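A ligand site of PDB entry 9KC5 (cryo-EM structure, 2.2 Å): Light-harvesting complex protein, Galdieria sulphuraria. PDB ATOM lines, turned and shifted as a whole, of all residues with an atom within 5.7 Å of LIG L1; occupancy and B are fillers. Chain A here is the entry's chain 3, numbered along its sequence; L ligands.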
ATOM      1  N   GLY A   1       8.345   2.717   9.739  1.00  0.00           N
ATOM      2  CA  GLY A   1       7.016   3.209  10.148  1.00  0.00           C
ATOM      3  C   GLY A   1       6.216   2.106  10.841  1.00  0.00           C
ATOM      4  O   GLY A   1       5.396   1.448  10.196  1.00  0.00           O
ATOM      5  N   PHE A   2       6.458   1.931  12.147  1.00  0.00           N
ATOM      6  CA  PHE A   2       5.792   0.914  12.940  1.00  0.00           C
ATOM      7  C   PHE A   2       5.182   1.578  14.184  1.00  0.00           C
ATOM      8  O   PHE A   2       5.848   1.717  15.209  1.00  0.00           O
ATOM      9  CB  PHE A   2       6.798  -0.189  13.273  1.00  0.00           C
ATOM     10  CG  PHE A   2       6.284  -1.311  14.163  1.00  0.00           C
ATOM     11  CD1 PHE A   2       5.283  -2.166  13.717  1.00  0.00           C
ATOM     12  CD2 PHE A   2       6.830  -1.546  15.427  1.00  0.00           C
ATOM     13  CE1 PHE A   2       4.811  -3.196  14.523  1.00  0.00           C
ATOM     14  CE2 PHE A   2       6.360  -2.584  16.221  1.00  0.00           C
ATOM     15  CZ  PHE A   2       5.357  -3.402  15.774  1.00  0.00           C
ATOM     16  N   ASP A   3       3.917   1.996  14.062  1.00  0.00           N
ATOM     17  CA  ASP A   3       3.139   2.504  15.181  1.00  0.00           C
ATOM     18  C   ASP A   3       1.678   2.105  15.004  1.00  0.00           C
ATOM     19  O   ASP A   3       0.844   2.950  14.697  1.00  0.00           O
ATOM     20  CB  ASP A   3       3.336   4.011  15.323  1.00  0.00           C
ATOM     21  CG  ASP A   3       2.838   4.625  16.619  1.00  0.00           C
ATOM     22  OD1 ASP A   3       2.410   3.866  17.519  1.00  0.00           O
ATOM     23  OD2 ASP A   3       2.875   5.873  16.727  1.00  0.00           O
ATOM     24  N   LEU A   5      -0.564   1.238  17.406  1.00  0.00           N
ATOM     25  CA  LEU A   5      -1.396   1.772  18.464  1.00  0.00           C
ATOM     26  C   LEU A   5      -1.556   3.290  18.308  1.00  0.00           C
ATOM     27  O   LEU A   5      -2.658   3.809  18.470  1.00  0.00           O
ATOM     28  CB  LEU A   5      -0.821   1.398  19.830  1.00  0.00           C
ATOM     29  CG  LEU A   5      -0.804  -0.097  20.158  1.00  0.00           C
ATOM     30  CD1 LEU A   5       0.042  -0.392  21.396  1.00  0.00           C
ATOM     31  CD2 LEU A   5      -2.198  -0.653  20.357  1.00  0.00           C
ATOM     32  N   GLY A   6      -0.451   3.981  18.013  1.00  0.00           N
ATOM     33  CA  GLY A   6      -0.482   5.393  17.663  1.00  0.00           C
ATOM     34  C   GLY A   6      -0.072   6.279  18.836  1.00  0.00           C
ATOM     35  O   GLY A   6      -0.804   7.209  19.192  1.00  0.00           O
ATOM     36  N   PHE A   7       1.103   5.994  19.418  1.00  0.00           N
ATOM     37  CA  PHE A   7       1.635   6.754  20.533  1.00  0.00           C
ATOM     38  C   PHE A   7       2.322   8.030  20.031  1.00  0.00           C
ATOM     39  O   PHE A   7       2.361   9.028  20.753  1.00  0.00           O
ATOM     40  CB  PHE A   7       2.595   5.889  21.354  1.00  0.00           C
ATOM     41  CG  PHE A   7       1.914   4.955  22.339  1.00  0.00           C
ATOM     42  CD1 PHE A   7       1.292   3.786  21.911  1.00  0.00           C
ATOM     43  CD2 PHE A   7       1.904   5.243  23.706  1.00  0.00           C
ATOM     44  CE1 PHE A   7       0.666   2.942  22.815  1.00  0.00           C
ATOM     45  CE2 PHE A   7       1.284   4.386  24.611  1.00  0.00           C
ATOM     46  CZ  PHE A   7       0.669   3.241  24.167  1.00  0.00           C
ATOM     47  N   SER A   8       2.874   7.979  18.807  1.00  0.00           N
ATOM     48  CA  SER A   8       3.564   9.126  18.222  1.00  0.00           C
ATOM     49  C   SER A   8       2.598  10.261  17.899  1.00  0.00           C
ATOM     50  O   SER A   8       3.008  11.416  17.816  1.00  0.00           O
ATOM     51  CB  SER A   8       4.345   8.707  16.996  1.00  0.00           C
ATOM     52  OG  SER A   8       3.473   8.270  15.950  1.00  0.00           O
ATOM     53  N   LEU A  13       7.216  12.498  19.474  1.00  0.00           N
ATOM     54  CA  LEU A  13       8.097  11.440  19.013  1.00  0.00           C
ATOM     55  C   LEU A  13       9.510  11.644  19.565  1.00  0.00           C
ATOM     56  O   LEU A  13      10.221  10.669  19.823  1.00  0.00           O
ATOM     57  CB  LEU A  13       8.095  11.406  17.483  1.00  0.00           C
ATOM     58  CG  LEU A  13       8.836  10.242  16.814  1.00  0.00           C
ATOM     59  CD1 LEU A  13       8.206   8.898  17.110  1.00  0.00           C
ATOM     60  CD2 LEU A  13       8.922  10.459  15.311  1.00  0.00           C
ATOM     61  N   LEU A  16       9.461  10.136  22.949  1.00  0.00           N
ATOM     62  CA  LEU A  16       9.427   8.695  22.812  1.00  0.00           C
ATOM     63  C   LEU A  16      10.804   8.146  22.416  1.00  0.00           C
ATOM     64  O   LEU A  16      11.176   7.054  22.845  1.00  0.00           O
ATOM     65  CB  LEU A  16       8.347   8.308  21.803  1.00  0.00           C
ATOM     66  CG  LEU A  16       6.897   8.543  22.253  1.00  0.00           C
ATOM     67  CD1 LEU A  16       5.939   8.546  21.065  1.00  0.00           C
ATOM     68  CD2 LEU A  16       6.452   7.507  23.268  1.00  0.00           C
ATOM     69  N   ARG A  17      11.555   8.904  21.609  1.00  0.00           N
ATOM     70  CA  ARG A  17      12.882   8.508  21.176  1.00  0.00           C
ATOM     71  C   ARG A  17      13.843   8.513  22.358  1.00  0.00           C
ATOM     72  O   ARG A  17      14.657   7.590  22.499  1.00  0.00           O
ATOM     73  CB  ARG A  17      13.394   9.415  20.053  1.00  0.00           C
ATOM     74  CG  ARG A  17      14.836   9.185  19.606  1.00  0.00           C
ATOM     75  CD  ARG A  17      15.086   7.785  19.065  1.00  0.00           C
ATOM     76  NE  ARG A  17      14.458   7.600  17.746  1.00  0.00           N
ATOM     77  CZ  ARG A  17      14.224   6.438  17.153  1.00  0.00           C
ATOM     78  NH1 ARG A  17      13.712   6.416  15.929  1.00  0.00           N
ATOM     79  NH2 ARG A  17      14.502   5.303  17.755  1.00  0.00           N
ATOM     80  N   SER A  19      13.024   8.064  25.416  1.00  0.00           N
ATOM     81  CA  SER A  19      12.615   6.911  26.196  1.00  0.00           C
ATOM     82  C   SER A  19      13.140   5.613  25.580  1.00  0.00           C
ATOM     83  O   SER A  19      13.560   4.715  26.307  1.00  0.00           O
ATOM     84  CB  SER A  19      11.108   6.879  26.346  1.00  0.00           C
ATOM     85  OG  SER A  19      10.685   5.757  27.111  1.00  0.00           O
ATOM     86  N   GLU A  20      13.089   5.525  24.246  1.00  0.00           N
ATOM     87  CA  GLU A  20      13.532   4.344  23.526  1.00  0.00           C
ATOM     88  C   GLU A  20      15.032   4.124  23.702  1.00  0.00           C
ATOM     89  O   GLU A  20      15.468   3.045  24.087  1.00  0.00           O
ATOM     90  CB  GLU A  20      13.179   4.458  22.038  1.00  0.00           C
ATOM     91  CG  GLU A  20      13.425   3.169  21.251  1.00  0.00           C
ATOM     92  CD  GLU A  20      12.899   3.205  19.827  1.00  0.00           C
ATOM     93  OE1 GLU A  20      12.649   4.305  19.297  1.00  0.00           O
ATOM     94  OE2 GLU A  20      12.715   2.110  19.247  1.00  0.00           O
ATOM     95  N   HIS A  23      15.957   3.034  27.253  1.00  0.00           N
ATOM     96  CA  HIS A  23      15.680   1.619  27.418  1.00  0.00           C
ATOM     97  C   HIS A  23      16.757   0.777  26.738  1.00  0.00           C
ATOM     98  O   HIS A  23      17.234  -0.206  27.306  1.00  0.00           O
ATOM     99  CB  HIS A  23      14.299   1.237  26.875  1.00  0.00           C
ATOM    100  CG  HIS A  23      13.149   1.501  27.787  1.00  0.00           C
ATOM    101  ND1 HIS A  23      12.405   2.671  27.770  1.00  0.00           N
ATOM    102  CD2 HIS A  23      12.598   0.736  28.734  1.00  0.00           C
ATOM    103  CE1 HIS A  23      11.450   2.591  28.685  1.00  0.00           C
ATOM    104  NE2 HIS A  23      11.547   1.422  29.284  1.00  0.00           N
ATOM    105  N   LEU A 117      20.305   1.556  17.848  1.00  0.00           N
ATOM    106  CA  LEU A 117      18.858   1.376  17.972  1.00  0.00           C
ATOM    107  C   LEU A 117      18.467  -0.081  17.722  1.00  0.00           C
ATOM    108  O   LEU A 117      17.657  -0.624  18.472  1.00  0.00           O
ATOM    109  CB  LEU A 117      18.212   2.341  16.980  1.00  0.00           C
ATOM    110  CG  LEU A 117      16.681   2.311  16.881  1.00  0.00           C
ATOM    111  CD1 LEU A 117      16.017   2.484  18.237  1.00  0.00           C
ATOM    112  CD2 LEU A 117      16.235   3.397  15.921  1.00  0.00           C
ATOM    113  N   ARG A 121      17.152  -2.553  20.634  1.00  0.00           N
ATOM    114  CA  ARG A 121      15.838  -3.177  20.596  1.00  0.00           C
ATOM    115  C   ARG A 121      15.936  -4.678  20.862  1.00  0.00           C
ATOM    116  O   ARG A 121      15.082  -5.237  21.547  1.00  0.00           O
ATOM    117  CB  ARG A 121      15.157  -2.913  19.240  1.00  0.00           C
ATOM    118  CG  ARG A 121      14.610  -1.497  19.070  1.00  0.00           C
ATOM    119  CD  ARG A 121      14.363  -1.163  17.608  1.00  0.00           C
ATOM    120  NE  ARG A 121      13.788   0.180  17.425  1.00  0.00           N
ATOM    121  CZ  ARG A 121      13.587   0.791  16.254  1.00  0.00           C
ATOM    122  NH1 ARG A 121      13.056   1.999  16.225  1.00  0.00           N
ATOM    123  NH2 ARG A 121      13.916   0.194  15.111  1.00  0.00           N
ATOM    124  N   LEU A 122      16.971  -5.324  20.308  1.00  0.00           N
ATOM    125  CA  LEU A 122      17.205  -6.749  20.489  1.00  0.00           C
ATOM    126  C   LEU A 122      17.602  -7.040  21.935  1.00  0.00           C
ATOM    127  O   LEU A 122      17.150  -8.017  22.514  1.00  0.00           O
ATOM    128  CB  LEU A 122      18.290  -7.220  19.513  1.00  0.00           C
ATOM    129  CG  LEU A 122      17.917  -7.199  18.026  1.00  0.00           C
ATOM    130  CD1 LEU A 122      19.167  -7.316  17.174  1.00  0.00           C
ATOM    131  CD2 LEU A 122      16.937  -8.303  17.680  1.00  0.00           C
ATOM    132  N   MET A 124      16.838  -5.374  24.549  1.00  0.00           N
ATOM    133  CA  MET A 124      15.698  -5.118  25.417  1.00  0.00           C
ATOM    134  C   MET A 124      14.805  -6.355  25.528  1.00  0.00           C
ATOM    135  O   MET A 124      14.371  -6.699  26.622  1.00  0.00           O
ATOM    136  CB  MET A 124      14.888  -3.920  24.889  1.00  0.00           C
ATOM    137  CG  MET A 124      15.558  -2.587  25.157  1.00  0.00           C
ATOM    138  SD  MET A 124      15.025  -1.294  24.020  1.00  0.00           S
ATOM    139  CE  MET A 124      13.283  -1.234  24.427  1.00  0.00           C
ATOM    140  N   ILE A 125      14.536  -7.013  24.390  1.00  0.00           N
ATOM    141  CA  ILE A 125      13.768  -8.246  24.360  1.00  0.00           C
ATOM    142  C   ILE A 125      14.575  -9.354  25.041  1.00  0.00           C
ATOM    143  O   ILE A 125      14.002 -10.190  25.738  1.00  0.00           O
ATOM    144  CB  ILE A 125      13.361  -8.608  22.912  1.00  0.00           C
ATOM    145  CG1 ILE A 125      12.373  -7.591  22.346  1.00  0.00           C
ATOM    146  CG2 ILE A 125      12.805 -10.036  22.835  1.00  0.00           C
ATOM    147  CD1 ILE A 125      12.174  -7.670  20.844  1.00  0.00           C
HETATM  148 MG1  LIG L   1      10.306   1.362  19.338  1.00  0.00          MG
HETATM  149  C1  LIG L   1       9.513   3.050  16.415  1.00  0.00           C
HETATM  150  C2  LIG L   1       9.510   4.178  21.055  1.00  0.00           C
HETATM  151  C3  LIG L   1      10.670  -0.468  22.166  1.00  0.00           C
HETATM  152  C4  LIG L   1      10.779  -1.685  17.290  1.00  0.00           C
HETATM  153  N1  LIG L   1       9.603   3.250  18.854  1.00  0.00           N
HETATM  154  C5  LIG L   1       9.402   3.786  17.701  1.00  0.00           C
HETATM  155  C6  LIG L   1       8.982   5.231  17.688  1.00  0.00           C
HETATM  156  C7  LIG L   1       9.069   5.589  19.150  1.00  0.00           C
HETATM  157  C8  LIG L   1       9.419   4.244  19.729  1.00  0.00           C
HETATM  158  C9  LIG L   1      10.221   6.585  19.337  1.00  0.00           C
HETATM  159  C10 LIG L   1       7.528   5.400  17.214  1.00  0.00           C
HETATM  160  C11 LIG L   1       6.522   4.320  17.660  1.00  0.00           C
HETATM  161  C12 LIG L   1       6.042   4.504  19.081  1.00  0.00           C
HETATM  162  O1  LIG L   1       5.344   5.456  19.373  1.00  0.00           O
HETATM  163  O2  LIG L   1       6.404   3.546  20.120  1.00  0.00           O
HETATM  164  N2  LIG L   1      10.106   1.791  21.335  1.00  0.00           N
HETATM  165  C13 LIG L   1       9.843   2.993  21.850  1.00  0.00           C
HETATM  166  C14 LIG L   1       9.855   3.064  23.330  1.00  0.00           C
HETATM  167  C15 LIG L   1      10.205   1.675  23.712  1.00  0.00           C
HETATM  168  C16 LIG L   1      10.332   0.963  22.376  1.00  0.00           C
HETATM  169  C17 LIG L   1       9.601   4.261  24.216  1.00  0.00           C
HETATM  170  C18 LIG L   1      10.332   1.251  25.132  1.00  0.00           C
HETATM  171  C19 LIG L   1      10.526   0.029  25.582  1.00  0.00           C
HETATM  172  N3  LIG L   1      10.590  -0.658  19.634  1.00  0.00           N
HETATM  173  C20 LIG L   1      10.794  -1.177  20.871  1.00  0.00           C
HETATM  174  C21 LIG L   1      11.217  -2.608  20.849  1.00  0.00           C
HETATM  175  C22 LIG L   1      11.249  -2.955  19.423  1.00  0.00           C
HETATM  176  C23 LIG L   1      10.849  -1.683  18.766  1.00  0.00           C
HETATM  177  C24 LIG L   1      11.552  -3.529  21.989  1.00  0.00           C
HETATM  178  C25 LIG L   1      11.614  -4.281  18.785  1.00  0.00           C
HETATM  179  C26 LIG L   1      10.320  -4.971  18.395  1.00  0.00           C
HETATM  180  N4  LIG L   1      10.169   0.728  17.400  1.00  0.00           N
HETATM  181  C27 LIG L   1      10.425  -0.443  16.609  1.00  0.00           C
HETATM  182  C28 LIG L   1      10.297  -0.277  15.136  1.00  0.00           C
HETATM  183  C29 LIG L   1       9.917   1.164  15.079  1.00  0.00           C
HETATM  184  C30 LIG L   1       9.872   1.623  16.389  1.00  0.00           C
HETATM  185  C31 LIG L   1      10.447  -1.144  13.913  1.00  0.00           C
HETATM  186  C32 LIG L   1       9.565   2.301  14.185  1.00  0.00           C
HETATM  187  O3  LIG L   1       9.497   2.243  12.906  1.00  0.00           O
HETATM  188  C33 LIG L   1       9.305   3.512  15.016  1.00  0.00           C
HETATM  189  C34 LIG L   1      10.281   4.594  14.634  1.00  0.00           C
HETATM  190  O4  LIG L   1       9.880   5.726  14.400  1.00  0.00           O
HETATM  191  O5  LIG L   1      11.696   4.312  14.527  1.00  0.00           O
HETATM  192  C35 LIG L   1      12.343   4.341  13.261  1.00  0.00           C
HETATM  193  C36 LIG L   1       5.910   3.647  21.466  1.00  0.00           C
HETATM  194  C37 LIG L   1       6.166   2.358  22.218  1.00  0.00           C
HETATM  195  C38 LIG L   1       5.819   2.207  23.512  1.00  0.00           C
HETATM  196  C39 LIG L   1       5.138   3.320  24.261  1.00  0.00           C
HETATM  197  C40 LIG L   1       6.090   0.896  24.220  1.00  0.00           C
HETATM  198  C41 LIG L   1       4.892  -0.035  24.164  1.00  0.00           C
HETATM  199  C42 LIG L   1       4.048  -0.005  25.428  1.00  0.00           C
HETATM  200  C43 LIG L   1       2.935  -1.068  25.400  1.00  0.00           C
HETATM  201  C44 LIG L   1       1.654  -0.519  26.029  1.00  0.00           C
HETATM  202  C45 LIG L   1       3.440  -2.323  26.113  1.00  0.00           C
HETATM  203  C46 LIG L   1       2.492  -3.521  26.145  1.00  0.00           C
HETATM  204  C47 LIG L   1       2.026  -3.969  24.766  1.00  0.00           C
HETATM  205  C48 LIG L   1       1.772  -5.481  24.645  1.00  0.00           C
HETATM  206  C49 LIG L   1       1.008  -6.035  25.847  1.00  0.00           C
HETATM  207  C50 LIG L   1       3.088  -6.215  24.388  1.00  0.00           C
HETATM  208  C51 LIG L   1       2.982  -7.729  24.258  1.00  0.00           C
HETATM  209  C52 LIG L   1       1.985  -8.174  23.180  1.00  0.00           C
HETATM  210  C53 LIG L   1       2.287  -9.537  22.568  1.00  0.00           C
HETATM  211  C54 LIG L   1       2.634 -10.601  23.610  1.00  0.00           C
HETATM  212  C55 LIG L   1       3.377  -9.450  21.503  1.00  0.00           C
HETATM  213  C1  LG2 L   2      15.020  -3.215  30.393  1.00  0.00           C
HETATM  214  C2  LG2 L   2      14.572  -3.644  29.126  1.00  0.00           C
HETATM  215  C3  LG2 L   2      16.206  -4.052  30.913  1.00  0.00           C
HETATM  216  C4  LG2 L   2       7.857  -2.892  22.231  1.00  0.00           C
HETATM  217  C5  LG2 L   2      13.055  -3.399  28.886  1.00  0.00           C
HETATM  218  C6  LG2 L   2      19.555  -4.510  38.806  1.00  0.00           C
HETATM  219  C7  LG2 L   2      19.030  -5.855  35.819  1.00  0.00           C
HETATM  220  C8  LG2 L   2      18.976  -4.831  34.910  1.00  0.00           C
HETATM  221  C9  LG2 L   2      17.550  -4.608  34.325  1.00  0.00           C
HETATM  222  C10 LG2 L   2      12.655  -3.905  27.655  1.00  0.00           C
HETATM  223  C11 LG2 L   2      17.561  -4.425  32.922  1.00  0.00           C
HETATM  224  C12 LG2 L   2      16.152  -4.293  32.281  1.00  0.00           C
HETATM  225  C13 LG2 L   2       3.767  -3.292  19.225  1.00  0.00           C
HETATM  226  C14 LG2 L   2       3.857  -1.881  19.829  1.00  0.00           C
HETATM  227  C15 LG2 L   2       2.857  -0.953  19.027  1.00  0.00           C
HETATM  228  C16 LG2 L   2      11.265  -5.086  25.301  1.00  0.00           C
HETATM  229  C17 LG2 L   2       3.118   0.571  19.245  1.00  0.00           C
HETATM  230  C18 LG2 L   2       4.579   0.912  18.922  1.00  0.00           C
HETATM  231  C19 LG2 L   2       5.584  -0.027  19.522  1.00  0.00           C
HETATM  232  C20 LG2 L   2       5.278  -1.331  19.691  1.00  0.00           C
HETATM  233  C21 LG2 L   2       7.700  -4.372  21.884  1.00  0.00           C
HETATM  234  C22 LG2 L   2       6.405  -2.233  20.328  1.00  0.00           C
HETATM  235  C23 LG2 L   2       6.778  -1.931  21.612  1.00  0.00           C
HETATM  236  C24 LG2 L   2      11.302  -3.348  27.141  1.00  0.00           C
HETATM  237  C25 LG2 L   2       3.397  -1.915  21.285  1.00  0.00           C
HETATM  238  C26 LG2 L   2      10.885  -3.693  25.828  1.00  0.00           C
HETATM  239  C27 LG2 L   2       9.418  -3.252  25.589  1.00  0.00           C
HETATM  240  C28 LG2 L   2       8.783  -3.705  24.442  1.00  0.00           C
HETATM  241  C29 LG2 L   2       8.073  -2.605  23.606  1.00  0.00           C
HETATM  242  C30 LG2 L   2       6.936   0.195  18.838  1.00  0.00           C
HETATM  243  C31 LG2 L   2      22.260  -5.623  35.571  1.00  0.00           C
HETATM  244  C32 LG2 L   2      21.265  -6.532  36.299  1.00  0.00           C
HETATM  245  C33 LG2 L   2      20.236  -5.835  36.801  1.00  0.00           C
HETATM  246  C34 LG2 L   2      19.796  -5.922  38.262  1.00  0.00           C
HETATM  247  C35 LG2 L   2      20.958  -6.559  39.109  1.00  0.00           C
HETATM  248  C36 LG2 L   2      21.495  -7.879  38.467  1.00  0.00           C
HETATM  249  C37 LG2 L   2      22.057  -7.551  37.090  1.00  0.00           C
HETATM  250  O1  LG2 L   2      22.486  -8.413  39.259  1.00  0.00           O
HETATM  251  C38 LG2 L   2      18.520  -6.757  38.484  1.00  0.00           C
HETATM  252  O2  LG2 L   2       2.295   1.307  18.423  1.00  0.00           O
HETATM  253  C39 LG2 L   2      15.305  -1.706  30.450  1.00  0.00           C
HETATM  254  C40 LG2 L   2      16.783  -3.534  35.106  1.00  0.00           C
HETATM  255 MG1  LG3 L   3       9.698   0.690  30.873  1.00  0.00          MG
HETATM  256  C1  LG3 L   3       8.607   3.950  31.200  1.00  0.00           C
HETATM  257  C2  LG3 L   3       7.356   0.263  28.451  1.00  0.00           C
HETATM  258  C3  LG3 L   3      10.408  -2.622  31.005  1.00  0.00           C
HETATM  259  C4  LG3 L   3      11.861   1.246  33.840  1.00  0.00           C
HETATM  260  N1  LG3 L   3       8.223   1.872  29.994  1.00  0.00           N
HETATM  261  C5  LG3 L   3       8.009   3.128  30.110  1.00  0.00           C
HETATM  262  C6  LG3 L   3       7.050   3.764  29.129  1.00  0.00           C
HETATM  263  C7  LG3 L   3       6.638   2.554  28.308  1.00  0.00           C
HETATM  264  C8  LG3 L   3       7.463   1.489  28.970  1.00  0.00           C
HETATM  265  C9  LG3 L   3       5.133   2.324  28.459  1.00  0.00           C
HETATM  266  C10 LG3 L   3       7.743   4.788  28.230  1.00  0.00           C
HETATM  267  C11 LG3 L   3       6.779   5.533  27.301  1.00  0.00           C
HETATM  268  C12 LG3 L   3       6.036   6.613  28.047  1.00  0.00           C
HETATM  269  O1  LG3 L   3       6.634   7.557  28.535  1.00  0.00           O
HETATM  270  O2  LG3 L   3       4.591   6.557  28.172  1.00  0.00           O
HETATM  271  N2  LG3 L   3       9.010  -0.934  29.840  1.00  0.00           N
HETATM  272  C13 LG3 L   3       8.057  -0.948  28.910  1.00  0.00           C
HETATM  273  C14 LG3 L   3       7.702  -2.302  28.400  1.00  0.00           C
HETATM  274  C15 LG3 L   3       8.629  -3.178  29.171  1.00  0.00           C
HETATM  275  C16 LG3 L   3       9.383  -2.204  30.020  1.00  0.00           C
HETATM  276  C17 LG3 L   3       6.661  -2.623  27.359  1.00  0.00           C
HETATM  277  C18 LG3 L   3       8.824  -4.663  29.205  1.00  0.00           C
HETATM  278  C19 LG3 L   3       8.047  -5.526  28.570  1.00  0.00           C
HETATM  279  N3  LG3 L   3      10.856  -0.431  32.167  1.00  0.00           N
HETATM  280  C20 LG3 L   3      11.052  -1.753  31.999  1.00  0.00           C
HETATM  281  C21 LG3 L   3      12.008  -2.367  32.973  1.00  0.00           C
HETATM  282  C22 LG3 L   3      12.432  -1.221  33.798  1.00  0.00           C
HETATM  283  C23 LG3 L   3      11.670  -0.085  33.217  1.00  0.00           C
HETATM  284  C24 LG3 L   3      12.443  -3.804  33.079  1.00  0.00           C
HETATM  285  C25 LG3 L   3      13.413  -1.210  34.962  1.00  0.00           C
HETATM  286  C26 LG3 L   3      14.713  -0.640  34.442  1.00  0.00           C
HETATM  287  N4  LG3 L   3      10.181   2.149  32.219  1.00  0.00           N
HETATM  288  C27 LG3 L   3      11.023   2.356  33.371  1.00  0.00           C
HETATM  289  C28 LG3 L   3      10.942   3.703  34.003  1.00  0.00           C
HETATM  290  C29 LG3 L   3       9.937   4.321  33.106  1.00  0.00           C
HETATM  291  C30 LG3 L   3       9.568   3.382  32.151  1.00  0.00           C
HETATM  292  C31 LG3 L   3      11.568   4.399  35.177  1.00  0.00           C
HETATM  293  C32 LG3 L   3       9.160   5.557  32.818  1.00  0.00           C
HETATM  294  O3  LG3 L   3       9.246   6.632  33.511  1.00  0.00           O
HETATM  295  C33 LG3 L   3       8.294   5.338  31.636  1.00  0.00           C
HETATM  296  C34 LG3 L   3       6.856   5.482  32.048  1.00  0.00           C
HETATM  297  O4  LG3 L   3       6.385   4.823  32.967  1.00  0.00           O
HETATM  298  O5  LG3 L   3       5.992   6.429  31.359  1.00  0.00           O
HETATM  299  C35 LG3 L   3       5.016   7.170  32.082  1.00  0.00           C
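Asp 3 touches LIG L1.
Phe 7 touches LIG L1.
Ser 8 touches LIG L1.
CD1 of Leu 13 touches C10 of LIG L1, at 3.6 Å.
Leu 16 touches LIG L1.
Ser 19 touches LIG L1.
His 23 touches LIG L1 (ND1 to C18, 3.6 Å).
Met 124 touches LIG L1 (CE to C19, 3.2 Å).
Hydrophobic or aromatic side chains that line LIG L1: Phe 2, Phe 7, Leu 13, Leu 16, His 23 and Met 124.
Within 4 Å of LIG L1: Gly 1, Phe 2, Asp 3, Phe 7, Ser 8, Leu 13, Leu 16, Arg 17, Ser 19, Glu 20, His 23, Arg 121 and Met 124.
The nearest printed residue that does not touch LIG L1 is Ile 125 (4.005 Å).
MG1 of LIG L1 is bound by OE2 of Glu 20 (2.5 Å).
The backbone NH (N) of Phe 2 lies within hydrogen-bond range of an oxygen (O3) of LIG L1, at 3.1 Å.
NH1 of Arg 121 is in hydrogen-bond range of O5 of LIG L1.
O5 of LIG L1 is in hydrogen-bond range of NH1 of Arg 17.
The backbone NH of Gly 1 is in hydrogen-bond range of an oxygen (O3) of LIG L1, 3.4 Å away.
OD1 of Asp 3 is in hydrogen-bond range of O2 of LG2 L2, 2.7 Å away.
O2 of LG2 L2 is in hydrogen-bond range of N of Leu 5, at 3.0 Å.
MG1 of LG3 L3 is bound by NE2 of His 23, 2.5 Å away.
The side-chain carboxylate of Glu 20 lies within salt-bridge range of the guanidinium group of Arg 121, at 3.9 Å.
OE1 of Glu 20 is in salt-bridge range of NH2 of Arg 17 (2.6 Å).
The backbone NH (N) of Phe 7 is in hydrogen-bond range of the side-chain carboxylate (OD1) of Asp 3, at 3.1 Å.
O of Ser 19 lies within hydrogen-bond range of ND1 of His 23, 2.8 Å away.
The side-chain hydroxyl (OG) of Ser 8 sits at hydrogen-bond distance from the side-chain carboxylate (OD2) of Asp 3 (2.6 Å).
The backbone NH (N) of Gly 6 is in hydrogen-bond range of the side-chain carboxylate (OD1) of Asp 3.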
